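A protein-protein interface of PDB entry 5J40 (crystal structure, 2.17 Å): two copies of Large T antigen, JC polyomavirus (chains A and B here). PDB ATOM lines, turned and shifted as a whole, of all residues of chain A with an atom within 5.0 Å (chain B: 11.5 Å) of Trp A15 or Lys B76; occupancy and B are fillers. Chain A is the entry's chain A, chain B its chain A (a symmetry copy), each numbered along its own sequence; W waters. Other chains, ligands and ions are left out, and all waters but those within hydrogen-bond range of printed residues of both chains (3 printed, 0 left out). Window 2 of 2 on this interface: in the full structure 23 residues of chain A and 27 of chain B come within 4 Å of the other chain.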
ATOM      1  N   GLN A  12       3.434  -1.278  13.996  1.00  0.00           N
ATOM      2  CA  GLN A  12       2.462  -0.220  14.283  1.00  0.00           C
ATOM      3  C   GLN A  12       2.410   0.127  15.783  1.00  0.00           C
ATOM      4  O   GLN A  12       2.272  -0.769  16.615  1.00  0.00           O
ATOM      5  CB  GLN A  12       1.064  -0.637  13.761  1.00  0.00           C
ATOM      6  CG  GLN A  12      -0.055   0.385  14.013  1.00  0.00           C
ATOM      7  CD  GLN A  12       0.194   1.703  13.328  1.00  0.00           C
ATOM      8  OE1 GLN A  12       0.203   1.801  12.094  1.00  0.00           O
ATOM      9  NE2 GLN A  12       0.411   2.744  14.123  1.00  0.00           N
ATOM     10  N   VAL A  13       2.499   1.423  16.113  1.00  0.00           N
ATOM     11  CA  VAL A  13       2.418   1.902  17.497  1.00  0.00           C
ATOM     12  C   VAL A  13       0.985   1.766  17.983  1.00  0.00           C
ATOM     13  O   VAL A  13       0.053   2.073  17.241  1.00  0.00           O
ATOM     14  CB  VAL A  13       2.990   3.347  17.689  1.00  0.00           C
ATOM     15  CG1 VAL A  13       2.335   4.346  16.743  1.00  0.00           C
ATOM     16  CG2 VAL A  13       2.873   3.822  19.138  1.00  0.00           C
ATOM     17  N   SER A  14       0.801   1.279  19.207  1.00  0.00           N
ATOM     18  CA  SER A  14      -0.533   1.166  19.774  1.00  0.00           C
ATOM     19  C   SER A  14      -0.880   2.531  20.377  1.00  0.00           C
ATOM     20  O   SER A  14      -0.322   2.916  21.414  1.00  0.00           O
ATOM     21  CB  SER A  14      -0.592   0.068  20.833  1.00  0.00           C
ATOM     22  OG  SER A  14      -1.809   0.182  21.548  1.00  0.00           O
ATOM     23  N   TRP A  15      -1.789   3.263  19.705  1.00  0.00           N
ATOM     24  CA  TRP A  15      -2.287   4.568  20.142  1.00  0.00           C
ATOM     25  C   TRP A  15      -3.037   4.379  21.458  1.00  0.00           C
ATOM     26  O   TRP A  15      -2.953   5.235  22.348  1.00  0.00           O
ATOM     27  CB  TRP A  15      -3.222   5.174  19.064  1.00  0.00           C
ATOM     28  CG  TRP A  15      -2.532   5.663  17.811  1.00  0.00           C
ATOM     29  CD1 TRP A  15      -1.627   4.980  17.041  1.00  0.00           C
ATOM     30  CD2 TRP A  15      -2.778   6.900  17.136  1.00  0.00           C
ATOM     31  NE1 TRP A  15      -1.261   5.740  15.953  1.00  0.00           N
ATOM     32  CE2 TRP A  15      -1.958   6.920  15.982  1.00  0.00           C
ATOM     33  CE3 TRP A  15      -3.618   8.004  17.393  1.00  0.00           C
ATOM     34  CZ2 TRP A  15      -1.956   7.995  15.089  1.00  0.00           C
ATOM     35  CZ3 TRP A  15      -3.588   9.083  16.519  1.00  0.00           C
ATOM     36  CH2 TRP A  15      -2.772   9.068  15.385  1.00  0.00           C
ATOM     37  N   LYS A  16      -3.782   3.245  21.575  1.00  0.00           N
ATOM     38  CA  LYS A  16      -4.567   2.870  22.768  1.00  0.00           C
ATOM     39  C   LYS A  16      -3.660   2.748  24.008  1.00  0.00           C
ATOM     40  O   LYS A  16      -3.997   3.299  25.051  1.00  0.00           O
ATOM     41  CB  LYS A  16      -5.362   1.579  22.497  1.00  0.00           C
ATOM     42  CG  LYS A  16      -6.402   1.222  23.545  1.00  0.00           C
ATOM     43  CD  LYS A  16      -7.390   0.151  23.056  1.00  0.00           C
ATOM     44  CE  LYS A  16      -6.919  -1.272  23.232  1.00  0.00           C
ATOM     45  NZ  LYS A  16      -6.010  -1.701  22.141  1.00  0.00           N
ATOM     46  N   LEU A  17      -2.484   2.096  23.881  1.00  0.00           N
ATOM     47  CA  LEU A  17      -1.514   1.989  24.985  1.00  0.00           C
ATOM     48  C   LEU A  17      -0.937   3.365  25.371  1.00  0.00           C
ATOM     49  O   LEU A  17      -0.648   3.592  26.538  1.00  0.00           O
ATOM     50  CB  LEU A  17      -0.352   1.049  24.613  1.00  0.00           C
ATOM     51  CG  LEU A  17      -0.155  -0.289  25.349  1.00  0.00           C
ATOM     52  CD1 LEU A  17       1.262  -0.782  25.145  1.00  0.00           C
ATOM     53  CD2 LEU A  17      -0.439  -0.188  26.862  1.00  0.00           C
ATOM     54  N   VAL A  18      -0.737   4.273  24.408  1.00  0.00           N
ATOM     55  CA  VAL A  18      -0.205   5.620  24.737  1.00  0.00           C
ATOM     56  C   VAL A  18      -1.294   6.358  25.549  1.00  0.00           C
ATOM     57  O   VAL A  18      -0.992   7.016  26.544  1.00  0.00           O
ATOM     58  CB  VAL A  18       0.281   6.448  23.497  1.00  0.00           C
ATOM     59  CG1 VAL A  18       0.833   7.809  23.917  1.00  0.00           C
ATOM     60  CG2 VAL A  18       1.348   5.685  22.707  1.00  0.00           C
ATOM     61  N   THR A  19      -2.553   6.222  25.105  1.00  0.00           N
ATOM     62  CA  THR A  19      -3.736   6.795  25.739  1.00  0.00           C
ATOM     63  C   THR A  19      -3.890   6.302  27.174  1.00  0.00           C
ATOM     64  O   THR A  19      -4.108   7.108  28.076  1.00  0.00           O
ATOM     65  CB  THR A  19      -4.965   6.516  24.858  1.00  0.00           C
ATOM     66  OG1 THR A  19      -4.889   7.337  23.678  1.00  0.00           O
ATOM     67  CG2 THR A  19      -6.262   6.748  25.594  1.00  0.00           C
ATOM     68  N   ASN A  77       4.541  10.309  13.301  1.00  0.00           N
ATOM     69  CA  ASN A  77       3.301  10.984  13.684  1.00  0.00           C
ATOM     70  C   ASN A  77       3.148  11.053  15.215  1.00  0.00           C
ATOM     71  O   ASN A  77       2.062  10.818  15.729  1.00  0.00           O
ATOM     72  CB  ASN A  77       2.130  10.199  13.042  1.00  0.00           C
ATOM     73  CG  ASN A  77       0.878  10.999  12.840  1.00  0.00           C
ATOM     74  OD1 ASN A  77      -0.225  10.461  12.911  1.00  0.00           O
ATOM     75  ND2 ASN A  77       1.008  12.305  12.617  1.00  0.00           N
ATOM     76  N   SER A  80       0.583  13.687  16.850  1.00  0.00           N
ATOM     77  CA  SER A  80      -0.822  13.278  16.679  1.00  0.00           C
ATOM     78  C   SER A  80      -1.223  12.188  17.674  1.00  0.00           C
ATOM     79  O   SER A  80      -2.337  12.230  18.195  1.00  0.00           O
ATOM     80  CB  SER A  80      -1.081  12.783  15.261  1.00  0.00           C
ATOM     81  OG  SER A  80      -1.034  13.866  14.355  1.00  0.00           O
ATOM     82  N   ILE A  81      -0.337  11.185  17.892  1.00  0.00           N
ATOM     83  CA  ILE A  81      -0.600  10.074  18.820  1.00  0.00           C
ATOM     84  C   ILE A  81      -0.848  10.655  20.204  1.00  0.00           C
ATOM     85  O   ILE A  81      -1.765  10.226  20.887  1.00  0.00           O
ATOM     86  CB  ILE A  81       0.570   9.027  18.852  1.00  0.00           C
ATOM     87  CG1 ILE A  81       0.827   8.388  17.483  1.00  0.00           C
ATOM     88  CG2 ILE A  81       0.336   7.945  19.927  1.00  0.00           C
ATOM     89  CD1 ILE A  81       2.203   7.913  17.299  1.00  0.00           C
ATOM     90  N   GLN A  84      -4.212  12.766  20.546  1.00  0.00           N
ATOM     91  CA  GLN A  84      -5.378  11.915  20.785  1.00  0.00           C
ATOM     92  C   GLN A  84      -5.395  11.445  22.247  1.00  0.00           C
ATOM     93  O   GLN A  84      -6.454  11.474  22.884  1.00  0.00           O
ATOM     94  CB  GLN A  84      -5.475  10.736  19.809  1.00  0.00           C
ATOM     95  CG  GLN A  84      -6.729   9.878  20.069  1.00  0.00           C
ATOM     96  CD  GLN A  84      -6.980   8.868  18.996  1.00  0.00           C
ATOM     97  OE1 GLN A  84      -7.460   9.193  17.916  1.00  0.00           O
ATOM     98  NE2 GLN A  84      -6.739   7.607  19.298  1.00  0.00           N
ATOM     99  N   THR B  10      -7.999  -4.704   8.656  1.00  0.00           N
ATOM    100  CA  THR B  10      -8.434  -4.369  10.013  1.00  0.00           C
ATOM    101  C   THR B  10      -9.911  -3.953  10.070  1.00  0.00           C
ATOM    102  O   THR B  10     -10.475  -3.491   9.067  1.00  0.00           O
ATOM    103  CB  THR B  10      -7.512  -3.305  10.631  1.00  0.00           C
ATOM    104  N   LYS B  11     -10.535  -4.129  11.261  1.00  0.00           N
ATOM    105  CA  LYS B  11     -11.932  -3.777  11.533  1.00  0.00           C
ATOM    106  C   LYS B  11     -12.146  -2.271  11.389  1.00  0.00           C
ATOM    107  O   LYS B  11     -11.258  -1.488  11.724  1.00  0.00           O
ATOM    108  CB  LYS B  11     -12.353  -4.251  12.931  1.00  0.00           C
ATOM    109  CG  LYS B  11     -12.696  -5.733  12.992  1.00  0.00           C
ATOM    110  CD  LYS B  11     -13.095  -6.172  14.390  1.00  0.00           C
ATOM    111  CE  LYS B  11     -13.577  -7.601  14.402  1.00  0.00           C
ATOM    112  NZ  LYS B  11     -14.045  -8.022  15.748  1.00  0.00           N
ATOM    113  N   GLN B  12     -13.305  -1.877  10.860  1.00  0.00           N
ATOM    114  CA  GLN B  12     -13.673  -0.480  10.621  1.00  0.00           C
ATOM    115  C   GLN B  12     -14.778  -0.001  11.583  1.00  0.00           C
ATOM    116  O   GLN B  12     -15.808  -0.661  11.712  1.00  0.00           O
ATOM    117  CB  GLN B  12     -14.105  -0.297   9.144  1.00  0.00           C
ATOM    118  CG  GLN B  12     -14.533   1.129   8.765  1.00  0.00           C
ATOM    119  CD  GLN B  12     -13.424   2.134   8.932  1.00  0.00           C
ATOM    120  OE1 GLN B  12     -12.404   2.098   8.230  1.00  0.00           O
ATOM    121  NE2 GLN B  12     -13.600   3.049   9.877  1.00  0.00           N
ATOM    122  N   VAL B  13     -14.564   1.153  12.230  1.00  0.00           N
ATOM    123  CA  VAL B  13     -15.547   1.752  13.140  1.00  0.00           C
ATOM    124  C   VAL B  13     -16.704   2.301  12.323  1.00  0.00           C
ATOM    125  O   VAL B  13     -16.484   2.909  11.277  1.00  0.00           O
ATOM    126  CB  VAL B  13     -14.929   2.816  14.109  1.00  0.00           C
ATOM    127  CG1 VAL B  13     -14.176   3.903  13.351  1.00  0.00           C
ATOM    128  CG2 VAL B  13     -15.983   3.433  15.029  1.00  0.00           C
ATOM    129  N   SER B  14     -17.934   2.064  12.774  1.00  0.00           N
ATOM    130  CA  SER B  14     -19.098   2.599  12.086  1.00  0.00           C
ATOM    131  C   SER B  14     -19.299   4.030  12.594  1.00  0.00           C
ATOM    132  O   SER B  14     -19.714   4.233  13.743  1.00  0.00           O
ATOM    133  CB  SER B  14     -20.335   1.744  12.350  1.00  0.00           C
ATOM    134  OG  SER B  14     -21.482   2.444  11.906  1.00  0.00           O
ATOM    135  N   TRP B  15     -18.981   5.015  11.731  1.00  0.00           N
ATOM    136  CA  TRP B  15     -19.148   6.442  12.010  1.00  0.00           C
ATOM    137  C   TRP B  15     -20.636   6.727  12.182  1.00  0.00           C
ATOM    138  O   TRP B  15     -21.017   7.544  13.029  1.00  0.00           O
ATOM    139  CB  TRP B  15     -18.562   7.286  10.847  1.00  0.00           C
ATOM    140  CG  TRP B  15     -17.053   7.301  10.757  1.00  0.00           C
ATOM    141  CD1 TRP B  15     -16.209   6.222  10.768  1.00  0.00           C
ATOM    142  CD2 TRP B  15     -16.230   8.450  10.537  1.00  0.00           C
ATOM    143  NE1 TRP B  15     -14.905   6.637  10.616  1.00  0.00           N
ATOM    144  CE2 TRP B  15     -14.889   8.000  10.463  1.00  0.00           C
ATOM    145  CE3 TRP B  15     -16.492   9.829  10.392  1.00  0.00           C
ATOM    146  CZ2 TRP B  15     -13.821   8.874  10.249  1.00  0.00           C
ATOM    147  CZ3 TRP B  15     -15.423  10.696  10.212  1.00  0.00           C
ATOM    148  CH2 TRP B  15     -14.112  10.218  10.137  1.00  0.00           C
ATOM    149  N   MET B  34     -16.815  11.560  22.919  1.00  0.00           N
ATOM    150  CA  MET B  34     -15.602  10.749  22.920  1.00  0.00           C
ATOM    151  C   MET B  34     -15.517   9.953  24.236  1.00  0.00           C
ATOM    152  O   MET B  34     -15.378   8.731  24.216  1.00  0.00           O
ATOM    153  CB  MET B  34     -14.404  11.690  22.757  1.00  0.00           C
ATOM    154  CG  MET B  34     -13.100  11.001  22.476  1.00  0.00           C
ATOM    155  SD  MET B  34     -11.888  12.174  21.769  1.00  0.00           S
ATOM    156  CE  MET B  34     -10.427  11.251  22.019  1.00  0.00           C
ATOM    157  N   LEU B  38     -16.140   5.841  24.582  1.00  0.00           N
ATOM    158  CA  LEU B  38     -15.084   4.994  25.098  1.00  0.00           C
ATOM    159  C   LEU B  38     -15.558   4.167  26.282  1.00  0.00           C
ATOM    160  O   LEU B  38     -15.123   3.025  26.422  1.00  0.00           O
ATOM    161  CB  LEU B  38     -13.846   5.811  25.468  1.00  0.00           C
ATOM    162  CG  LEU B  38     -13.006   6.212  24.260  1.00  0.00           C
ATOM    163  CD1 LEU B  38     -12.155   7.447  24.562  1.00  0.00           C
ATOM    164  CD2 LEU B  38     -12.162   5.042  23.777  1.00  0.00           C
ATOM    165  N   GLN B  41     -16.747   0.426  25.807  1.00  0.00           N
ATOM    166  CA  GLN B  41     -15.789  -0.575  25.331  1.00  0.00           C
ATOM    167  C   GLN B  41     -15.637  -1.861  26.205  1.00  0.00           C
ATOM    168  O   GLN B  41     -15.148  -2.862  25.684  1.00  0.00           O
ATOM    169  CB  GLN B  41     -14.421   0.063  25.066  1.00  0.00           C
ATOM    170  CG  GLN B  41     -13.572   0.335  26.314  1.00  0.00           C
ATOM    171  CD  GLN B  41     -12.205   0.847  25.945  1.00  0.00           C
ATOM    172  OE1 GLN B  41     -11.916   2.038  26.060  1.00  0.00           O
ATOM    173  NE2 GLN B  41     -11.325  -0.048  25.501  1.00  0.00           N
ATOM    174  N   ASN B  68     -18.804  -1.773  18.523  1.00  0.00           N
ATOM    175  CA  ASN B  68     -18.337  -0.591  17.794  1.00  0.00           C
ATOM    176  C   ASN B  68     -17.390   0.244  18.667  1.00  0.00           C
ATOM    177  O   ASN B  68     -16.422   0.795  18.160  1.00  0.00           O
ATOM    178  CB  ASN B  68     -19.521   0.241  17.297  1.00  0.00           C
ATOM    179  CG  ASN B  68     -19.207   1.201  16.178  1.00  0.00           C
ATOM    180  OD1 ASN B  68     -18.517   0.865  15.230  1.00  0.00           O
ATOM    181  ND2 ASN B  68     -19.744   2.414  16.238  1.00  0.00           N
ATOM    182  N   ALA B  69     -17.648   0.295  19.984  1.00  0.00           N
ATOM    183  CA  ALA B  69     -16.856   1.042  20.958  1.00  0.00           C
ATOM    184  C   ALA B  69     -15.511   0.399  21.168  1.00  0.00           C
ATOM    185  O   ALA B  69     -14.522   1.103  21.375  1.00  0.00           O
ATOM    186  CB  ALA B  69     -17.603   1.162  22.268  1.00  0.00           C
ATOM    187  N   GLN B  70     -15.455  -0.941  21.067  1.00  0.00           N
ATOM    188  CA  GLN B  70     -14.192  -1.664  21.146  1.00  0.00           C
ATOM    189  C   GLN B  70     -13.333  -1.265  19.949  1.00  0.00           C
ATOM    190  O   GLN B  70     -12.167  -0.943  20.142  1.00  0.00           O
ATOM    191  CB  GLN B  70     -14.433  -3.174  21.131  1.00  0.00           C
ATOM    192  CG  GLN B  70     -14.932  -3.694  22.459  1.00  0.00           C
ATOM    193  CD  GLN B  70     -15.009  -5.193  22.460  1.00  0.00           C
ATOM    194  OE1 GLN B  70     -15.559  -5.822  21.551  1.00  0.00           O
ATOM    195  NE2 GLN B  70     -14.504  -5.795  23.520  1.00  0.00           N
ATOM    196  N   ILE B  71     -13.933  -1.222  18.715  1.00  0.00           N
ATOM    197  CA  ILE B  71     -13.235  -0.832  17.480  1.00  0.00           C
ATOM    198  C   ILE B  71     -12.820   0.632  17.578  1.00  0.00           C
ATOM    199  O   ILE B  71     -11.705   0.969  17.188  1.00  0.00           O
ATOM    200  CB  ILE B  71     -14.069  -1.124  16.190  1.00  0.00           C
ATOM    201  CG1 ILE B  71     -14.494  -2.601  16.129  1.00  0.00           C
ATOM    202  CG2 ILE B  71     -13.280  -0.730  14.917  1.00  0.00           C
ATOM    203  CD1 ILE B  71     -15.664  -2.889  15.117  1.00  0.00           C
ATOM    204  N   PHE B  72     -13.710   1.488  18.115  1.00  0.00           N
ATOM    205  CA  PHE B  72     -13.455   2.905  18.340  1.00  0.00           C
ATOM    206  C   PHE B  72     -12.237   3.117  19.261  1.00  0.00           C
ATOM    207  O   PHE B  72     -11.458   4.057  19.035  1.00  0.00           O
ATOM    208  CB  PHE B  72     -14.710   3.584  18.915  1.00  0.00           C
ATOM    209  CG  PHE B  72     -14.555   5.071  19.178  1.00  0.00           C
ATOM    210  CD1 PHE B  72     -14.703   5.997  18.147  1.00  0.00           C
ATOM    211  CD2 PHE B  72     -14.282   5.545  20.467  1.00  0.00           C
ATOM    212  CE1 PHE B  72     -14.560   7.366  18.394  1.00  0.00           C
ATOM    213  CE2 PHE B  72     -14.159   6.914  20.716  1.00  0.00           C
ATOM    214  CZ  PHE B  72     -14.294   7.815  19.681  1.00  0.00           C
ATOM    215  N   ALA B  73     -12.047   2.228  20.269  1.00  0.00           N
ATOM    216  CA  ALA B  73     -10.910   2.319  21.199  1.00  0.00           C
ATOM    217  C   ALA B  73      -9.561   2.093  20.474  1.00  0.00           C
ATOM    218  O   ALA B  73      -8.526   2.597  20.933  1.00  0.00           O
ATOM    219  CB  ALA B  73     -11.073   1.320  22.339  1.00  0.00           C
ATOM    220  N   ASP B  74      -9.588   1.335  19.350  1.00  0.00           N
ATOM    221  CA  ASP B  74      -8.418   1.031  18.513  1.00  0.00           C
ATOM    222  C   ASP B  74      -8.195   2.063  17.384  1.00  0.00           C
ATOM    223  O   ASP B  74      -7.179   1.971  16.681  1.00  0.00           O
ATOM    224  CB  ASP B  74      -8.555  -0.380  17.892  1.00  0.00           C
ATOM    225  CG  ASP B  74      -8.494  -1.523  18.893  1.00  0.00           C
ATOM    226  OD1 ASP B  74      -7.679  -1.443  19.842  1.00  0.00           O
ATOM    227  OD2 ASP B  74      -9.241  -2.513  18.710  1.00  0.00           O
ATOM    228  N   SER B  75      -9.142   3.021  17.199  1.00  0.00           N
ATOM    229  CA  SER B  75      -9.081   4.048  16.150  1.00  0.00           C
ATOM    230  C   SER B  75      -7.983   5.103  16.370  1.00  0.00           C
ATOM    231  O   SER B  75      -7.715   5.506  17.501  1.00  0.00           O
ATOM    232  CB  SER B  75     -10.448   4.719  15.971  1.00  0.00           C
ATOM    233  OG  SER B  75     -10.441   5.695  14.935  1.00  0.00           O
ATOM    234  N   LYS B  76      -7.365   5.550  15.263  1.00  0.00           N
ATOM    235  CA  LYS B  76      -6.335   6.600  15.218  1.00  0.00           C
ATOM    236  C   LYS B  76      -6.996   7.924  14.785  1.00  0.00           C
ATOM    237  O   LYS B  76      -6.307   8.907  14.513  1.00  0.00           O
ATOM    238  CB  LYS B  76      -5.273   6.239  14.183  1.00  0.00           C
ATOM    239  CG  LYS B  76      -4.470   4.979  14.486  1.00  0.00           C
ATOM    240  CD  LYS B  76      -3.658   4.615  13.248  1.00  0.00           C
ATOM    241  CE  LYS B  76      -2.900   3.333  13.407  1.00  0.00           C
ATOM    242  NZ  LYS B  76      -3.792   2.159  13.556  1.00  0.00           N
ATOM    243  N   ASN B  77      -8.337   7.947  14.703  1.00  0.00           N
ATOM    244  CA  ASN B  77      -9.046   9.127  14.209  1.00  0.00           C
ATOM    245  C   ASN B  77     -10.318   9.405  15.031  1.00  0.00           C
ATOM    246  O   ASN B  77     -11.355   9.717  14.460  1.00  0.00           O
ATOM    247  CB  ASN B  77      -9.389   8.871  12.720  1.00  0.00           C
ATOM    248  CG  ASN B  77      -9.597  10.112  11.904  1.00  0.00           C
ATOM    249  OD1 ASN B  77     -10.391  10.117  10.966  1.00  0.00           O
ATOM    250  ND2 ASN B  77      -8.919  11.203  12.255  1.00  0.00           N
ATOM    251  N   GLN B  78     -10.249   9.211  16.370  1.00  0.00           N
ATOM    252  CA  GLN B  78     -11.402   9.355  17.275  1.00  0.00           C
ATOM    253  C   GLN B  78     -12.051  10.737  17.257  1.00  0.00           C
ATOM    254  O   GLN B  78     -13.275  10.826  17.274  1.00  0.00           O
ATOM    255  CB  GLN B  78     -11.004   8.999  18.730  1.00  0.00           C
ATOM    256  CG  GLN B  78     -10.516   7.567  18.880  1.00  0.00           C
ATOM    257  CD  GLN B  78     -10.124   7.250  20.283  1.00  0.00           C
ATOM    258  OE1 GLN B  78      -9.780   8.124  21.089  1.00  0.00           O
ATOM    259  NE2 GLN B  78     -10.160   5.993  20.611  1.00  0.00           N
ATOM    260  N   LYS B  79     -11.241  11.815  17.330  1.00  0.00           N
ATOM    261  CA  LYS B  79     -11.790  13.177  17.336  1.00  0.00           C
ATOM    262  C   LYS B  79     -12.553  13.477  16.047  1.00  0.00           C
ATOM    263  O   LYS B  79     -13.608  14.095  16.123  1.00  0.00           O
ATOM    264  CB  LYS B  79     -10.728  14.253  17.599  1.00  0.00           C
ATOM    265  CG  LYS B  79     -11.382  15.574  18.041  1.00  0.00           C
ATOM    266  CD  LYS B  79     -10.391  16.684  18.265  1.00  0.00           C
ATOM    267  CE  LYS B  79     -11.045  17.909  18.857  1.00  0.00           C
ATOM    268  NZ  LYS B  79     -10.164  19.106  18.752  1.00  0.00           N
ATOM    269  N   SER B  80     -12.042  13.037  14.880  1.00  0.00           N
ATOM    270  CA  SER B  80     -12.754  13.265  13.611  1.00  0.00           C
ATOM    271  C   SER B  80     -14.111  12.561  13.584  1.00  0.00           C
ATOM    272  O   SER B  80     -15.075  13.134  13.079  1.00  0.00           O
ATOM    273  CB  SER B  80     -11.922  12.797  12.423  1.00  0.00           C
ATOM    274  OG  SER B  80     -10.818  13.658  12.237  1.00  0.00           O
ATOM    275  N   ILE B  81     -14.169  11.299  14.077  1.00  0.00           N
ATOM    276  CA  ILE B  81     -15.409  10.509  14.107  1.00  0.00           C
ATOM    277  C   ILE B  81     -16.443  11.272  14.922  1.00  0.00           C
ATOM    278  O   ILE B  81     -17.593  11.353  14.521  1.00  0.00           O
ATOM    279  CB  ILE B  81     -15.191   9.066  14.687  1.00  0.00           C
ATOM    280  CG1 ILE B  81     -14.184   8.249  13.869  1.00  0.00           C
ATOM    281  CG2 ILE B  81     -16.525   8.304  14.834  1.00  0.00           C
ATOM    282  CD1 ILE B  81     -13.499   7.208  14.643  1.00  0.00           C
ATOM    283  N   CYS B  82     -16.031  11.797  16.077  1.00  0.00           N
ATOM    284  CA  CYS B  82     -16.893  12.536  17.002  1.00  0.00           C
ATOM    285  C   CYS B  82     -17.305  13.903  16.478  1.00  0.00           C
ATOM    286  O   CYS B  82     -18.412  14.335  16.759  1.00  0.00           O
ATOM    287  CB  CYS B  82     -16.248  12.620  18.387  1.00  0.00           C
ATOM    288  SG  CYS B  82     -16.085  11.012  19.203  1.00  0.00           S
HETATM  289  O   HOH W   1      -8.333  11.696  17.450  1.00  0.00           O
HETATM  290  O   HOH W   2      -4.485   1.837  18.635  1.00  0.00           O
HETATM  291  O   HOH W   3      -5.067  -0.889  19.476  1.00  0.00           O
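Trp A15 touches just one residue of chain B: Lys B76 (3.4 Å). Of chain A, only Gln A12, Trp A15 and Gln A84 come within 4 Å of Lys B76. No residue of chain B comes within 4 Å of Val A13. Of chain B, only Ala B73 and Asp B74 come within 4 Å of Lys A16. No residue of chain B comes within 4 Å of Thr A19. No residue of chain B comes within 4 Å of Asn A77. No residue of chain B comes within 4 Å of Ile A81. Of chain B, only Ser B75 (2.9 Å), Lys B76 (3.4 Å), Asn B77 (3.6 Å) and Gln B78 (3.2 Å) come within 4 Å of Gln A84. Of the printed residues of chain A, Asp B74 touches Lys A16. Printed residues of chain A within 4 Å of Asn B77: Gln A84 (3.6 Å). Phe B72 touches none of the printed residues of chain A. The nearest printed residue of chain A that does not touch Lys B76 is Val A13 (5.0 Å).
Water W1 lies within hydrogen-bond range of OE1 of Gln A84 (2.7 Å), N of Lys B79 (2.9 Å) and N of Gln B78 (3.3 Å). Water W3 lies within hydrogen-bond range of OD1 of Asp B74 (2.7 Å) and NZ of Lys A16 (2.9 Å). Water W2 lies within hydrogen-bond range of N of Trp A15, O of Asp B74 and N of Lys A16.
The backbone carbonyl oxygen of Gln B78 is in hydrogen-bond range of the side-chain sulfur of Cys B82 (3.4 Å). NE2 of Gln B78 sits at hydrogen-bond distance from O of Phe B72 (2.8 Å). O of Trp A15 lies within hydrogen-bond range of OG1 of Thr A19. OG of Ser B75 lies within hydrogen-bond range of N of Asn B77 (3.1 Å). OG of Ser B80 lies within hydrogen-bond range of ND2 of Asn B77 (3.1 Å).
The side-chain amino group (NZ) of Lys A16 lies within salt-bridge range of the side-chain carboxylate (OD1) of Asp B74 (2.9 Å). The side-chain amide nitrogen of Gln A84 lies within hydrogen-bond range of the backbone carbonyl oxygen of Ser B75. The backbone NH (N) of Gln B78 sits at hydrogen-bond distance from the side-chain amide oxygen (OE1) of Gln A84 (3.2 Å).
7 positions are printed for both chains. Of the 8 pairs that touch across the chains among the printed residues, none has its exchanged pair printed and touching as well.
Of the 12 printed residues of chain A, 4 touch a printed residue of chain B. Among the printed residues, 8 pairs touch across the chains. Among the printed residues, Asp or Glu carboxylates within 4 Å of a Lys or Arg side-chain nitrogen of the other chain: Lys A16 with Asp B74 (2.9 Å).
Among the printed residues, pairs that only touch across the chains: Gln A12 with Lys B76, Trp A15 with Lys B76, Lys A16 with Ala B73, Gln A84 with Lys B76 and Gln A84 with Asn B77.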
